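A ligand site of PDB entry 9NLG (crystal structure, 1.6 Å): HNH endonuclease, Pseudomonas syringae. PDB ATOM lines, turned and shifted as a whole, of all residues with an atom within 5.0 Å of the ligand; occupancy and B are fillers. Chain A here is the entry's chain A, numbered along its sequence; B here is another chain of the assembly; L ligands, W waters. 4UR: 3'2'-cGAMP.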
ATOM      1  N   HIS A 138      -1.811  14.162 -15.954  1.00  0.00           N
ATOM      2  CA  HIS A 138      -1.108  15.175 -15.190  1.00  0.00           C
ATOM      3  C   HIS A 138      -0.850  16.446 -15.987  1.00  0.00           C
ATOM      4  O   HIS A 138      -0.462  17.465 -15.414  1.00  0.00           O
ATOM      5  CB  HIS A 138       0.197  14.610 -14.612  1.00  0.00           C
ATOM      6  CG  HIS A 138       1.357  14.566 -15.560  1.00  0.00           C
ATOM      7  ND1 HIS A 138       1.456  13.653 -16.580  1.00  0.00           N
ATOM      8  CD2 HIS A 138       2.482  15.316 -15.607  1.00  0.00           C
ATOM      9  CE1 HIS A 138       2.590  13.839 -17.232  1.00  0.00           C
ATOM     10  NE2 HIS A 138       3.229  14.844 -16.661  1.00  0.00           N
ATOM     11  N   PHE A 139      -1.124  16.426 -17.287  1.00  0.00           N
ATOM     12  CA  PHE A 139      -1.033  17.627 -18.086  1.00  0.00           C
ATOM     13  C   PHE A 139      -2.275  18.484 -17.866  1.00  0.00           C
ATOM     14  O   PHE A 139      -3.318  17.995 -17.423  1.00  0.00           O
ATOM     15  CB  PHE A 139      -0.913  17.287 -19.567  1.00  0.00           C
ATOM     16  CG  PHE A 139       0.173  16.319 -19.887  1.00  0.00           C
ATOM     17  CD1 PHE A 139       1.459  16.759 -20.101  1.00  0.00           C
ATOM     18  CD2 PHE A 139      -0.081  14.962 -19.997  1.00  0.00           C
ATOM     19  CE1 PHE A 139       2.466  15.888 -20.397  1.00  0.00           C
ATOM     20  CE2 PHE A 139       0.944  14.087 -20.280  1.00  0.00           C
ATOM     21  CZ  PHE A 139       2.211  14.553 -20.505  1.00  0.00           C
ATOM     22  N   LEU A 216       2.236   7.673 -22.749  1.00  0.00           N
ATOM     23  CA  LEU A 216       2.336   9.137 -22.712  1.00  0.00           C
ATOM     24  C   LEU A 216       1.829   9.516 -21.313  1.00  0.00           C
ATOM     25  O   LEU A 216       0.622   9.693 -21.101  1.00  0.00           O
ATOM     26  CB  LEU A 216       1.556   9.813 -23.825  1.00  0.00           C
ATOM     27  CG  LEU A 216       2.124  11.173 -24.254  1.00  0.00           C
ATOM     28  CD1 LEU A 216       1.420  11.657 -25.518  1.00  0.00           C
ATOM     29  CD2 LEU A 216       1.984  12.202 -23.139  1.00  0.00           C
ATOM     30  N   ALA A 217       2.752   9.589 -20.369  1.00  0.00           N
ATOM     31  CA  ALA A 217       2.447   9.643 -18.943  1.00  0.00           C
ATOM     32  C   ALA A 217       3.667  10.195 -18.227  1.00  0.00           C
ATOM     33  O   ALA A 217       4.714  10.439 -18.840  1.00  0.00           O
ATOM     34  CB  ALA A 217       2.061   8.256 -18.410  1.00  0.00           C
ATOM     35  N   ASP A 218       3.517  10.410 -16.916  1.00  0.00           N
ATOM     36  CA  ASP A 218       4.617  10.953 -16.122  1.00  0.00           C
ATOM     37  C   ASP A 218       5.886  10.146 -16.377  1.00  0.00           C
ATOM     38  O   ASP A 218       5.850   8.916 -16.420  1.00  0.00           O
ATOM     39  CB  ASP A 218       4.297  10.885 -14.624  1.00  0.00           C
ATOM     40  CG  ASP A 218       2.842  11.158 -14.294  1.00  0.00           C
ATOM     41  OD1 ASP A 218       1.936  10.480 -14.834  1.00  0.00           O
ATOM     42  OD2 ASP A 218       2.600  12.022 -13.425  1.00  0.00           O
ATOM     43  N   ILE A 219       7.015  10.845 -16.530  1.00  0.00           N
ATOM     44  CA  ILE A 219       8.289  10.142 -16.728  1.00  0.00           C
ATOM     45  C   ILE A 219       8.539   9.105 -15.632  1.00  0.00           C
ATOM     46  O   ILE A 219       8.901   7.965 -15.959  1.00  0.00           O
ATOM     47  CB  ILE A 219       9.438  11.148 -16.872  1.00  0.00           C
ATOM     48  CG1 ILE A 219       9.326  11.870 -18.214  1.00  0.00           C
ATOM     49  CG2 ILE A 219      10.763  10.413 -16.756  1.00  0.00           C
ATOM     50  CD1 ILE A 219      10.271  13.033 -18.365  1.00  0.00           C
ATOM     51  N   LEU A 222       6.283   6.131 -16.336  1.00  0.00           N
ATOM     52  CA  LEU A 222       6.690   5.314 -17.477  1.00  0.00           C
ATOM     53  C   LEU A 222       7.909   4.459 -17.147  1.00  0.00           C
ATOM     54  O   LEU A 222       8.032   3.324 -17.640  1.00  0.00           O
ATOM     55  CB  LEU A 222       6.992   6.214 -18.665  1.00  0.00           C
ATOM     56  CG  LEU A 222       5.778   6.900 -19.288  1.00  0.00           C
ATOM     57  CD1 LEU A 222       6.246   7.895 -20.324  1.00  0.00           C
ATOM     58  CD2 LEU A 222       4.824   5.867 -19.869  1.00  0.00           C
ATOM     59  N   PHE A 240       4.294   7.790 -29.381  1.00  0.00           N
ATOM     60  CA  PHE A 240       3.429   8.868 -29.806  1.00  0.00           C
ATOM     61  C   PHE A 240       4.316  10.044 -30.200  1.00  0.00           C
ATOM     62  O   PHE A 240       5.187  10.452 -29.421  1.00  0.00           O
ATOM     63  CB  PHE A 240       2.474   9.286 -28.685  1.00  0.00           C
ATOM     64  CG  PHE A 240       1.451  10.323 -29.117  1.00  0.00           C
ATOM     65  CD1 PHE A 240       1.779  11.681 -29.163  1.00  0.00           C
ATOM     66  CD2 PHE A 240       0.162   9.956 -29.448  1.00  0.00           C
ATOM     67  CE1 PHE A 240       0.860  12.623 -29.552  1.00  0.00           C
ATOM     68  CE2 PHE A 240      -0.773  10.904 -29.828  1.00  0.00           C
ATOM     69  CZ  PHE A 240      -0.424  12.243 -29.885  1.00  0.00           C
ATOM     70  N   HIS A 241       4.116  10.540 -31.409  1.00  0.00           N
ATOM     71  CA  HIS A 241       4.918  11.607 -31.999  1.00  0.00           C
ATOM     72  C   HIS A 241       4.029  12.809 -32.305  1.00  0.00           C
ATOM     73  O   HIS A 241       2.934  12.649 -32.849  1.00  0.00           O
ATOM     74  CB  HIS A 241       5.588  11.091 -33.286  1.00  0.00           C
ATOM     75  CG  HIS A 241       6.713  11.942 -33.763  1.00  0.00           C
ATOM     76  ND1 HIS A 241       6.545  12.947 -34.689  1.00  0.00           N
ATOM     77  CD2 HIS A 241       8.021  11.938 -33.432  1.00  0.00           C
ATOM     78  CE1 HIS A 241       7.717  13.532 -34.915  1.00  0.00           C
ATOM     79  NE2 HIS A 241       8.623  12.947 -34.153  1.00  0.00           N
ATOM     80  N   ARG A 242       4.510  14.007 -31.949  1.00  0.00           N
ATOM     81  CA  ARG A 242       3.666  15.182 -32.132  1.00  0.00           C
ATOM     82  C   ARG A 242       3.265  15.385 -33.595  1.00  0.00           C
ATOM     83  O   ARG A 242       2.148  15.847 -33.867  1.00  0.00           O
ATOM     84  CB  ARG A 242       4.361  16.436 -31.618  1.00  0.00           C
ATOM     85  CG  ARG A 242       4.380  16.541 -30.095  1.00  0.00           C
ATOM     86  CD  ARG A 242       5.372  17.594 -29.636  1.00  0.00           C
ATOM     87  NE  ARG A 242       5.285  17.819 -28.200  1.00  0.00           N
ATOM     88  CZ  ARG A 242       5.905  17.092 -27.285  1.00  0.00           C
ATOM     89  NH1 ARG A 242       6.612  16.023 -27.606  1.00  0.00           N
ATOM     90  NH2 ARG A 242       5.809  17.443 -26.011  1.00  0.00           N
ATOM     91  N   SER A 277      15.299  14.976 -24.950  1.00  0.00           N
ATOM     92  CA  SER A 277      14.247  15.852 -25.439  1.00  0.00           C
ATOM     93  C   SER A 277      14.656  17.314 -25.400  1.00  0.00           C
ATOM     94  O   SER A 277      14.209  18.122 -26.225  1.00  0.00           O
ATOM     95  CB  SER A 277      12.979  15.706 -24.575  1.00  0.00           C
ATOM     96  OG  SER A 277      12.512  14.385 -24.544  1.00  0.00           O
ATOM     97  N   ALA A 278      15.476  17.665 -24.424  1.00  0.00           N
ATOM     98  CA  ALA A 278      15.875  19.035 -24.177  1.00  0.00           C
ATOM     99  C   ALA A 278      17.109  18.997 -23.293  1.00  0.00           C
ATOM    100  O   ALA A 278      17.461  17.953 -22.733  1.00  0.00           O
ATOM    101  CB  ALA A 278      14.744  19.847 -23.529  1.00  0.00           C
ATOM    102  N   GLN A 279      17.755  20.150 -23.178  1.00  0.00           N
ATOM    103  CA  GLN A 279      18.922  20.293 -22.319  1.00  0.00           C
ATOM    104  C   GLN A 279      18.472  20.580 -20.898  1.00  0.00           C
ATOM    105  O   GLN A 279      17.890  21.629 -20.624  1.00  0.00           O
ATOM    106  CB  GLN A 279      19.810  21.425 -22.851  1.00  0.00           C
ATOM    107  CG  GLN A 279      21.003  21.734 -21.967  1.00  0.00           C
ATOM    108  CD  GLN A 279      21.912  20.543 -21.809  1.00  0.00           C
ATOM    109  OE1 GLN A 279      22.402  20.000 -22.804  1.00  0.00           O
ATOM    110  NE2 GLN A 279      22.134  20.119 -20.575  1.00  0.00           N
ATOM    111  N   VAL A 280      18.761  19.661 -19.979  1.00  0.00           N
ATOM    112  CA  VAL A 280      18.460  19.873 -18.562  1.00  0.00           C
ATOM    113  C   VAL A 280      19.480  20.868 -18.007  1.00  0.00           C
ATOM    114  O   VAL A 280      20.675  20.584 -18.045  1.00  0.00           O
ATOM    115  CB  VAL A 280      18.484  18.567 -17.761  1.00  0.00           C
ATOM    116  CG1 VAL A 280      18.306  18.854 -16.272  1.00  0.00           C
ATOM    117  CG2 VAL A 280      17.426  17.597 -18.249  1.00  0.00           C
ATOM    118  N   PRO A 281      19.062  22.027 -17.488  1.00  0.00           N
ATOM    119  CA  PRO A 281      20.051  22.976 -16.952  1.00  0.00           C
ATOM    120  C   PRO A 281      20.678  22.458 -15.669  1.00  0.00           C
ATOM    121  O   PRO A 281      19.981  22.009 -14.752  1.00  0.00           O
ATOM    122  CB  PRO A 281      19.233  24.254 -16.712  1.00  0.00           C
ATOM    123  CG  PRO A 281      17.965  24.062 -17.494  1.00  0.00           C
ATOM    124  CD  PRO A 281      17.699  22.583 -17.463  1.00  0.00           C
ATOM    125  N   TYR A 304      12.301  17.211 -29.052  1.00  0.00           N
ATOM    126  CA  TYR A 304      11.104  16.411 -28.808  1.00  0.00           C
ATOM    127  C   TYR A 304      10.823  15.413 -29.930  1.00  0.00           C
ATOM    128  O   TYR A 304      10.124  14.413 -29.692  1.00  0.00           O
ATOM    129  CB  TYR A 304       9.878  17.314 -28.664  1.00  0.00           C
ATOM    130  CG  TYR A 304       9.783  18.106 -27.388  1.00  0.00           C
ATOM    131  CD1 TYR A 304      10.752  18.039 -26.404  1.00  0.00           C
ATOM    132  CD2 TYR A 304       8.677  18.916 -27.153  1.00  0.00           C
ATOM    133  CE1 TYR A 304      10.622  18.776 -25.213  1.00  0.00           C
ATOM    134  CE2 TYR A 304       8.544  19.647 -26.006  1.00  0.00           C
ATOM    135  CZ  TYR A 304       9.513  19.568 -25.034  1.00  0.00           C
ATOM    136  OH  TYR A 304       9.355  20.284 -23.897  1.00  0.00           O
ATOM    137  N   ALA A 339      15.645  13.646 -15.889  1.00  0.00           N
ATOM    138  CA  ALA A 339      15.482  13.240 -17.274  1.00  0.00           C
ATOM    139  C   ALA A 339      14.514  14.140 -18.026  1.00  0.00           C
ATOM    140  O   ALA A 339      13.361  14.297 -17.615  1.00  0.00           O
ATOM    141  CB  ALA A 339      14.999  11.786 -17.363  1.00  0.00           C
ATOM    142  N   ALA A 340      14.990  14.713 -19.126  1.00  0.00           N
ATOM    143  CA  ALA A 340      14.149  15.294 -20.163  1.00  0.00           C
ATOM    144  C   ALA A 340      14.282  14.342 -21.351  1.00  0.00           C
ATOM    145  O   ALA A 340      15.188  14.484 -22.176  1.00  0.00           O
ATOM    146  CB  ALA A 340      14.579  16.703 -20.525  1.00  0.00           C
ATOM    147  N   ILE A 341      13.395  13.349 -21.409  1.00  0.00           N
ATOM    148  CA  ILE A 341      13.480  12.291 -22.426  1.00  0.00           C
ATOM    149  C   ILE A 341      12.098  12.009 -22.965  1.00  0.00           C
ATOM    150  O   ILE A 341      11.076  12.225 -22.304  1.00  0.00           O
ATOM    151  CB  ILE A 341      14.084  10.986 -21.864  1.00  0.00           C
ATOM    152  CG1 ILE A 341      13.233  10.426 -20.717  1.00  0.00           C
ATOM    153  CG2 ILE A 341      15.523  11.233 -21.414  1.00  0.00           C
ATOM    154  CD1 ILE A 341      13.767   9.108 -20.117  1.00  0.00           C
ATOM    155  N   PRO A 342      12.026  11.518 -24.209  1.00  0.00           N
ATOM    156  CA  PRO A 342      10.734  11.104 -24.767  1.00  0.00           C
ATOM    157  C   PRO A 342      10.126   9.943 -24.002  1.00  0.00           C
ATOM    158  O   PRO A 342      10.813   9.152 -23.332  1.00  0.00           O
ATOM    159  CB  PRO A 342      11.088  10.708 -26.207  1.00  0.00           C
ATOM    160  CG  PRO A 342      12.308  11.510 -26.522  1.00  0.00           C
ATOM    161  CD  PRO A 342      13.090  11.527 -25.238  1.00  0.00           C
ATOM    162  N   ALA A 343       8.795   9.819 -24.119  1.00  0.00           N
ATOM    163  CA  ALA A 343       8.061   8.837 -23.324  1.00  0.00           C
ATOM    164  C   ALA A 343       8.512   7.413 -23.618  1.00  0.00           C
ATOM    165  O   ALA A 343       8.659   6.600 -22.686  1.00  0.00           O
ATOM    166  CB  ALA A 343       6.568   8.995 -23.582  1.00  0.00           C
ATOM    167  N   ALA A 346      11.583   6.668 -21.734  1.00  0.00           N
ATOM    168  CA  ALA A 346      11.361   6.466 -20.305  1.00  0.00           C
ATOM    169  C   ALA A 346      10.935   5.035 -20.003  1.00  0.00           C
ATOM    170  O   ALA A 346      11.383   4.445 -19.024  1.00  0.00           O
ATOM    171  CB  ALA A 346      10.323   7.450 -19.783  1.00  0.00           C
ATOM    172  N   ASP A 365      11.541  14.882 -10.773  1.00  0.00           N
ATOM    173  CA  ASP A 365      10.730  15.367 -11.875  1.00  0.00           C
ATOM    174  C   ASP A 365      10.336  16.806 -11.624  1.00  0.00           C
ATOM    175  O   ASP A 365      10.308  17.274 -10.474  1.00  0.00           O
ATOM    176  CB  ASP A 365       9.470  14.507 -12.066  1.00  0.00           C
ATOM    177  CG  ASP A 365       8.883  14.626 -13.463  1.00  0.00           C
ATOM    178  OD1 ASP A 365       9.538  15.224 -14.353  1.00  0.00           O
ATOM    179  OD2 ASP A 365       7.759  14.132 -13.683  1.00  0.00           O
ATOM    180  N   ARG A 366      10.020  17.502 -12.718  1.00  0.00           N
ATOM    181  CA  ARG A 366       9.564  18.882 -12.639  1.00  0.00           C
ATOM    182  C   ARG A 366       8.261  18.973 -11.851  1.00  0.00           C
ATOM    183  O   ARG A 366       7.350  18.171 -12.038  1.00  0.00           O
ATOM    184  CB  ARG A 366       9.355  19.457 -14.036  1.00  0.00           C
ATOM    185  CG  ARG A 366      10.608  19.522 -14.906  1.00  0.00           C
ATOM    186  CD  ARG A 366      11.609  20.499 -14.306  1.00  0.00           C
ATOM    187  NE  ARG A 366      12.713  20.825 -15.211  1.00  0.00           N
ATOM    188  CZ  ARG A 366      13.576  21.810 -14.992  1.00  0.00           C
ATOM    189  NH1 ARG A 366      13.463  22.603 -13.945  1.00  0.00           N
ATOM    190  NH2 ARG A 366      14.570  22.000 -15.852  1.00  0.00           N
ATOM    191  N   PHE A 374      12.851  20.678  -9.800  1.00  0.00           N
ATOM    192  CA  PHE A 374      12.866  19.223  -9.661  1.00  0.00           C
ATOM    193  C   PHE A 374      12.597  18.850  -8.201  1.00  0.00           C
ATOM    194  O   PHE A 374      13.132  19.468  -7.265  1.00  0.00           O
ATOM    195  CB  PHE A 374      14.223  18.645 -10.095  1.00  0.00           C
ATOM    196  CG  PHE A 374      14.432  18.562 -11.582  1.00  0.00           C
ATOM    197  CD1 PHE A 374      13.823  17.558 -12.341  1.00  0.00           C
ATOM    198  CD2 PHE A 374      15.275  19.442 -12.234  1.00  0.00           C
ATOM    199  CE1 PHE A 374      14.031  17.494 -13.714  1.00  0.00           C
ATOM    200  CE2 PHE A 374      15.479  19.369 -13.605  1.00  0.00           C
ATOM    201  CZ  PHE A 374      14.862  18.395 -14.336  1.00  0.00           C
ATOM    202  N   ASP B 231      -0.874  19.240 -27.461  1.00  0.00           N
ATOM    203  CA  ASP B 231      -0.362  18.531 -28.633  1.00  0.00           C
ATOM    204  C   ASP B 231      -0.217  17.037 -28.384  1.00  0.00           C
ATOM    205  O   ASP B 231       0.627  16.375 -29.006  1.00  0.00           O
ATOM    206  CB  ASP B 231       0.971  19.139 -29.095  1.00  0.00           C
ATOM    207  CG  ASP B 231       2.024  19.169 -27.996  1.00  0.00           C
ATOM    208  OD1 ASP B 231       1.761  18.672 -26.885  1.00  0.00           O
ATOM    209  OD2 ASP B 231       3.120  19.702 -28.250  1.00  0.00           O
ATOM    210  N   ARG B 232      -1.073  16.477 -27.509  1.00  0.00           N
ATOM    211  CA  ARG B 232      -0.999  15.079 -27.092  1.00  0.00           C
ATOM    212  C   ARG B 232      -2.359  14.412 -27.244  1.00  0.00           C
ATOM    213  O   ARG B 232      -2.857  13.701 -26.377  1.00  0.00           O
ATOM    214  CB  ARG B 232      -0.508  14.968 -25.653  1.00  0.00           C
ATOM    215  CG  ARG B 232      -1.223  15.873 -24.649  1.00  0.00           C
ATOM    216  CD  ARG B 232      -0.482  15.922 -23.331  1.00  0.00           C
ATOM    217  NE  ARG B 232       0.870  16.446 -23.475  1.00  0.00           N
ATOM    218  CZ  ARG B 232       1.166  17.737 -23.608  1.00  0.00           C
ATOM    219  NH1 ARG B 232       0.228  18.670 -23.633  1.00  0.00           N
ATOM    220  NH2 ARG B 232       2.437  18.089 -23.736  1.00  0.00           N
ATOM    221  N   GLN B 321      11.363  24.326 -30.888  1.00  0.00           N
ATOM    222  CA  GLN B 321      11.665  23.650 -29.638  1.00  0.00           C
ATOM    223  C   GLN B 321      13.150  23.356 -29.504  1.00  0.00           C
ATOM    224  O   GLN B 321      13.689  23.410 -28.395  1.00  0.00           O
ATOM    225  CB  GLN B 321      10.859  22.358 -29.510  1.00  0.00           C
ATOM    226  CG  GLN B 321      11.009  21.714 -28.140  1.00  0.00           C
ATOM    227  CD  GLN B 321      12.165  20.723 -28.054  1.00  0.00           C
ATOM    228  OE1 GLN B 321      12.455  20.021 -29.012  1.00  0.00           O
ATOM    229  NE2 GLN B 321      12.811  20.673 -26.892  1.00  0.00           N
ATOM    230  N   GLU B 328      16.340  28.201 -23.043  1.00  0.00           N
ATOM    231  CA  GLU B 328      15.949  27.956 -21.660  1.00  0.00           C
ATOM    232  C   GLU B 328      17.134  27.544 -20.806  1.00  0.00           C
ATOM    233  O   GLU B 328      17.190  27.890 -19.627  1.00  0.00           O
ATOM    234  CB  GLU B 328      14.847  26.887 -21.602  1.00  0.00           C
ATOM    235  CG  GLU B 328      13.516  27.378 -22.167  1.00  0.00           C
ATOM    236  CD  GLU B 328      12.400  26.361 -22.020  1.00  0.00           C
ATOM    237  OE1 GLU B 328      12.620  25.341 -21.340  1.00  0.00           O
ATOM    238  OE2 GLU B 328      11.312  26.590 -22.601  1.00  0.00           O
ATOM    239  N   THR B 355       3.999  20.969 -21.717  1.00  0.00           N
ATOM    240  CA  THR B 355       4.601  19.932 -20.894  1.00  0.00           C
ATOM    241  C   THR B 355       4.450  20.294 -19.417  1.00  0.00           C
ATOM    242  O   THR B 355       4.093  21.424 -19.071  1.00  0.00           O
ATOM    243  CB  THR B 355       6.087  19.787 -21.225  1.00  0.00           C
ATOM    244  OG1 THR B 355       6.679  21.088 -21.303  1.00  0.00           O
ATOM    245  CG2 THR B 355       6.294  19.058 -22.527  1.00  0.00           C
ATOM    246  N   GLN B 356       4.742  19.320 -18.559  1.00  0.00           N
ATOM    247  CA  GLN B 356       4.879  19.614 -17.130  1.00  0.00           C
ATOM    248  C   GLN B 356       5.941  20.688 -16.914  1.00  0.00           C
ATOM    249  O   GLN B 356       5.730  21.658 -16.184  1.00  0.00           O
ATOM    250  CB  GLN B 356       5.227  18.336 -16.368  1.00  0.00           C
ATOM    251  CG  GLN B 356       5.543  18.531 -14.892  1.00  0.00           C
ATOM    252  CD  GLN B 356       4.317  18.579 -13.999  1.00  0.00           C
ATOM    253  OE1 GLN B 356       3.173  18.596 -14.488  1.00  0.00           O
ATOM    254  NE2 GLN B 356       4.524  18.570 -12.686  1.00  0.00           N
ATOM    255  N   HIS B 357       7.100  20.505 -17.535  1.00  0.00           N
ATOM    256  CA  HIS B 357       8.130  21.527 -17.509  1.00  0.00           C
ATOM    257  C   HIS B 357       7.586  22.839 -18.035  1.00  0.00           C
ATOM    258  O   HIS B 357       6.987  22.883 -19.131  1.00  0.00           O
ATOM    259  CB  HIS B 357       9.324  21.136 -18.338  1.00  0.00           C
ATOM    260  CG  HIS B 357      10.280  22.267 -18.530  1.00  0.00           C
ATOM    261  ND1 HIS B 357      11.021  22.765 -17.484  1.00  0.00           N
ATOM    262  CD2 HIS B 357      10.581  23.024 -19.608  1.00  0.00           C
ATOM    263  CE1 HIS B 357      11.767  23.759 -17.919  1.00  0.00           C
ATOM    264  NE2 HIS B 357      11.520  23.947 -19.204  1.00  0.00           N
HETATM  265  C21 4UR L   1       6.329  12.262 -20.777  1.00  0.00           C
HETATM  266  C22 4UR L   1       5.724  13.138 -19.708  1.00  0.00           C
HETATM  267  C28 4UR L   1       8.475  16.547 -20.244  1.00  0.00           C
HETATM  268  N01 4UR L   1      11.728  20.914 -22.293  1.00  0.00           N
HETATM  269  C02 4UR L   1      12.104  20.405 -21.112  1.00  0.00           C
HETATM  270  N03 4UR L   1      11.487  19.317 -20.636  1.00  0.00           N
HETATM  271  C04 4UR L   1      11.974  18.944 -19.432  1.00  0.00           C
HETATM  272  C05 4UR L   1      12.979  19.543 -18.698  1.00  0.00           C
HETATM  273  N06 4UR L   1      13.188  18.860 -17.499  1.00  0.00           N
HETATM  274  C07 4UR L   1      12.319  17.876 -17.532  1.00  0.00           C
HETATM  275  N08 4UR L   1      11.554  17.873 -18.687  1.00  0.00           N
HETATM  276  C09 4UR L   1      10.475  16.926 -19.014  1.00  0.00           C
HETATM  277  O10 4UR L   1      10.828  16.144 -20.124  1.00  0.00           O
HETATM  278  C11 4UR L   1       9.659  15.900 -20.951  1.00  0.00           C
HETATM  279  C12 4UR L   1       9.964  16.422 -22.335  1.00  0.00           C
HETATM  280  O13 4UR L   1       8.803  16.279 -23.185  1.00  0.00           O
HETATM  281  P14 4UR L   1       8.655  15.064 -24.227  1.00  0.00           P
HETATM  282  O15 4UR L   1       7.384  15.285 -24.994  1.00  0.00           O
HETATM  283  O16 4UR L   1       9.963  14.894 -24.964  1.00  0.00           O
HETATM  284  O17 4UR L   1       8.496  13.759 -23.291  1.00  0.00           O
HETATM  285  C18 4UR L   1       7.348  13.632 -22.447  1.00  0.00           C
HETATM  286  C19 4UR L   1       7.711  12.718 -21.272  1.00  0.00           C
HETATM  287  O20 4UR L   1       8.437  11.562 -21.685  1.00  0.00           O
HETATM  288  O23 4UR L   1       5.677  14.509 -20.164  1.00  0.00           O
HETATM  289  P24 4UR L   1       6.200  15.685 -19.193  1.00  0.00           P
HETATM  290  O25 4UR L   1       5.896  15.308 -17.770  1.00  0.00           O
HETATM  291  O26 4UR L   1       5.656  16.972 -19.742  1.00  0.00           O
HETATM  292  O27 4UR L   1       7.804  15.618 -19.380  1.00  0.00           O
HETATM  293  C29 4UR L   1       9.175  17.628 -19.407  1.00  0.00           C
HETATM  294  O30 4UR L   1       8.416  18.050 -18.292  1.00  0.00           O
HETATM  295  O31 4UR L   1       5.490  12.292 -21.959  1.00  0.00           O
HETATM  296  C32 4UR L   1       6.176  12.878 -23.048  1.00  0.00           C
HETATM  297  N33 4UR L   1       5.253  13.768 -23.756  1.00  0.00           N
HETATM  298  C34 4UR L   1       4.639  14.889 -23.246  1.00  0.00           C
HETATM  299  N35 4UR L   1       3.886  15.509 -24.114  1.00  0.00           N
HETATM  300  C36 4UR L   1       4.020  14.766 -25.273  1.00  0.00           C
HETATM  301  C37 4UR L   1       3.468  14.912 -26.563  1.00  0.00           C
HETATM  302  N38 4UR L   1       2.669  15.903 -26.913  1.00  0.00           N
HETATM  303  N39 4UR L   1       3.811  14.001 -27.500  1.00  0.00           N
HETATM  304  C40 4UR L   1       4.640  12.998 -27.155  1.00  0.00           C
HETATM  305  N41 4UR L   1       5.222  12.758 -25.976  1.00  0.00           N
HETATM  306  C42 4UR L   1       4.871  13.689 -25.068  1.00  0.00           C
HETATM  307  C43 4UR L   1      13.631  20.689 -19.202  1.00  0.00           C
HETATM  308  O44 4UR L   1      14.537  21.354 -18.675  1.00  0.00           O
HETATM  309  N45 4UR L   1      13.108  21.058 -20.444  1.00  0.00           N
HETATM  310  O   HOH W   1      15.203  23.960 -19.289  1.00  0.00           O
HETATM  311  O   HOH W   2      12.536  22.689 -24.770  1.00  0.00           O
HETATM  312  O   HOH W   3       7.649  11.502 -26.312  1.00  0.00           O
HETATM  313  O   HOH W   4       8.111  16.384 -16.213  1.00  0.00           O
HETATM  314  O   HOH W   5      13.909  23.189 -22.278  1.00  0.00           O
HETATM  315  O   HOH W   6       6.643  13.520 -15.783  1.00  0.00           O
HETATM  316  O   HOH W   7       9.330  13.467 -27.241  1.00  0.00           O
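An oxygen (O26) of the ligand is in hydrogen-bond range of the backbone NH of Gln 356 of chain B (2.8 Å).
The backbone NH of Ala 343 lies within hydrogen-bond range of an oxygen (O20) of the ligand (3.0 Å).
O of Asp 231 of chain B lies within hydrogen-bond range of N38 of the ligand, at 3.0 Å.
The guanidinium group of Arg 366 lies within hydrogen-bond range of an oxygen (O44) of the ligand, 2.9 Å away.
OH of Tyr 304 is in hydrogen-bond range of N01 of the ligand (2.9 Å).
O of Ile 341 is in hydrogen-bond range of O20 of the ligand.
N of His 357 of chain B is in hydrogen-bond range of O30 of the ligand, at 2.9 Å.
A ring nitrogen (NE2) of His 138 is in hydrogen-bond range of an oxygen (O25) of the ligand (2.9 Å).
N38 of the ligand sits at hydrogen-bond distance from OD1 of Asp 231 of chain B (2.9 Å).
OG of Ser 277 sits at hydrogen-bond distance from O16 of the ligand.
NH1 of Arg 242 is in salt-bridge range of O15 of the ligand.
A nitrogen (N35) of the ligand lies within hydrogen-bond range of the guanidinium group (NH2) of Arg 232 of chain B.
NE of Arg 242 lies within salt-bridge range of OD2 of Asp 231 of chain B.
The side-chain amide nitrogen (NE2) of Gln 356 of chain B is in hydrogen-bond range of the backbone carbonyl oxygen (O) of Arg 366, 2.9 Å away.
O of Ser 277 sits at hydrogen-bond distance from NE2 of Gln 321 of chain B (3.0 Å).
OD1 of Asp 231 of chain B is in salt-bridge range of NH2 of Arg 232 of chain B, 3.3 Å away.
OE1 of Glu 328 of chain B sits at hydrogen-bond distance from NE2 of His 357 of chain B, 2.8 Å away.
The guanidinium group (NE) of Arg 366 sits at hydrogen-bond distance from a ring nitrogen (ND1) of His 357 of chain B, at 3.4 Å.
The backbone NH of Ser 277 is in hydrogen-bond range of the backbone carbonyl oxygen of Ala 340, 2.8 Å away.
OE1 of Gln 321 of chain B is in hydrogen-bond range of N of Tyr 304 (2.8 Å).
Phe 139 touches the ligand (CE1 to O26, 3.4 Å).
Leu 216 touches the ligand.
O of Ala 217 touches C22 of the ligand (3.0 Å).
CG1 of Ile 219 touches C19 of the ligand (3.6 Å).
Phe 240 touches the ligand (O to C40, 3.5 Å).
Ala 278 touches the ligand (CB to N01, 3.4 Å).
Gln 279 touches the ligand (O to O44, 3.9 Å).
Pro 281 touches the ligand (CD to O44, 3.6 Å).
Ala 339 touches the ligand.
Ala 340 touches the ligand (CA to O10, 3.4 Å).
Pro 342 touches the ligand (C to O20, 3.3 Å).
Phe 374 touches the ligand.
CB of Thr 355 of chain B touches O26 of the ligand, at 3.2 Å.
24 residues have an atom within 4 Å of the ligand: His 138, Phe 139, Leu 216, Ala 217, Ile 219, Phe 240, Arg 242, Ser 277, Ala 278, Gln 279, Pro 281, Tyr 304, Ala 339, Ala 340, Ile 341, Pro 342, Ala 343, Arg 366, Phe 374, Asp 231 of chain B, Arg 232 of chain B, Thr 355 of chain B, Gln 356 of chain B and His 357 of chain B.
Along chain A the residues within 4 Å of the ligand span positions 138 to 374.
Water W4 bridges the side-chain carboxylate (OD1) of Asp 365 and an oxygen (O30) of the ligand.
Water W3 bridges N41 of the ligand (2.8 Å) and N of Ala 343 (3.0 Å).
Water W7 bridges O of Tyr 304 and O16 of the ligand.
Water W6 lies within hydrogen-bond range of the side-chain carboxylate of Asp 365 (2.5 Å), an oxygen (O25) of the ligand (2.8 Å) and the backbone NH of Ile 219 (2.8 Å).
Water W5 lies within hydrogen-bond range of the side-chain carboxylate of Glu 328 of chain B (2.7 Å) and a nitrogen (N45) of the ligand (2.9 Å).
Water W2 bridges the side-chain amide nitrogen (NE2) of Gln 321 of chain B (2.9 Å) and a nitrogen (N01) of the ligand (3.2 Å).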
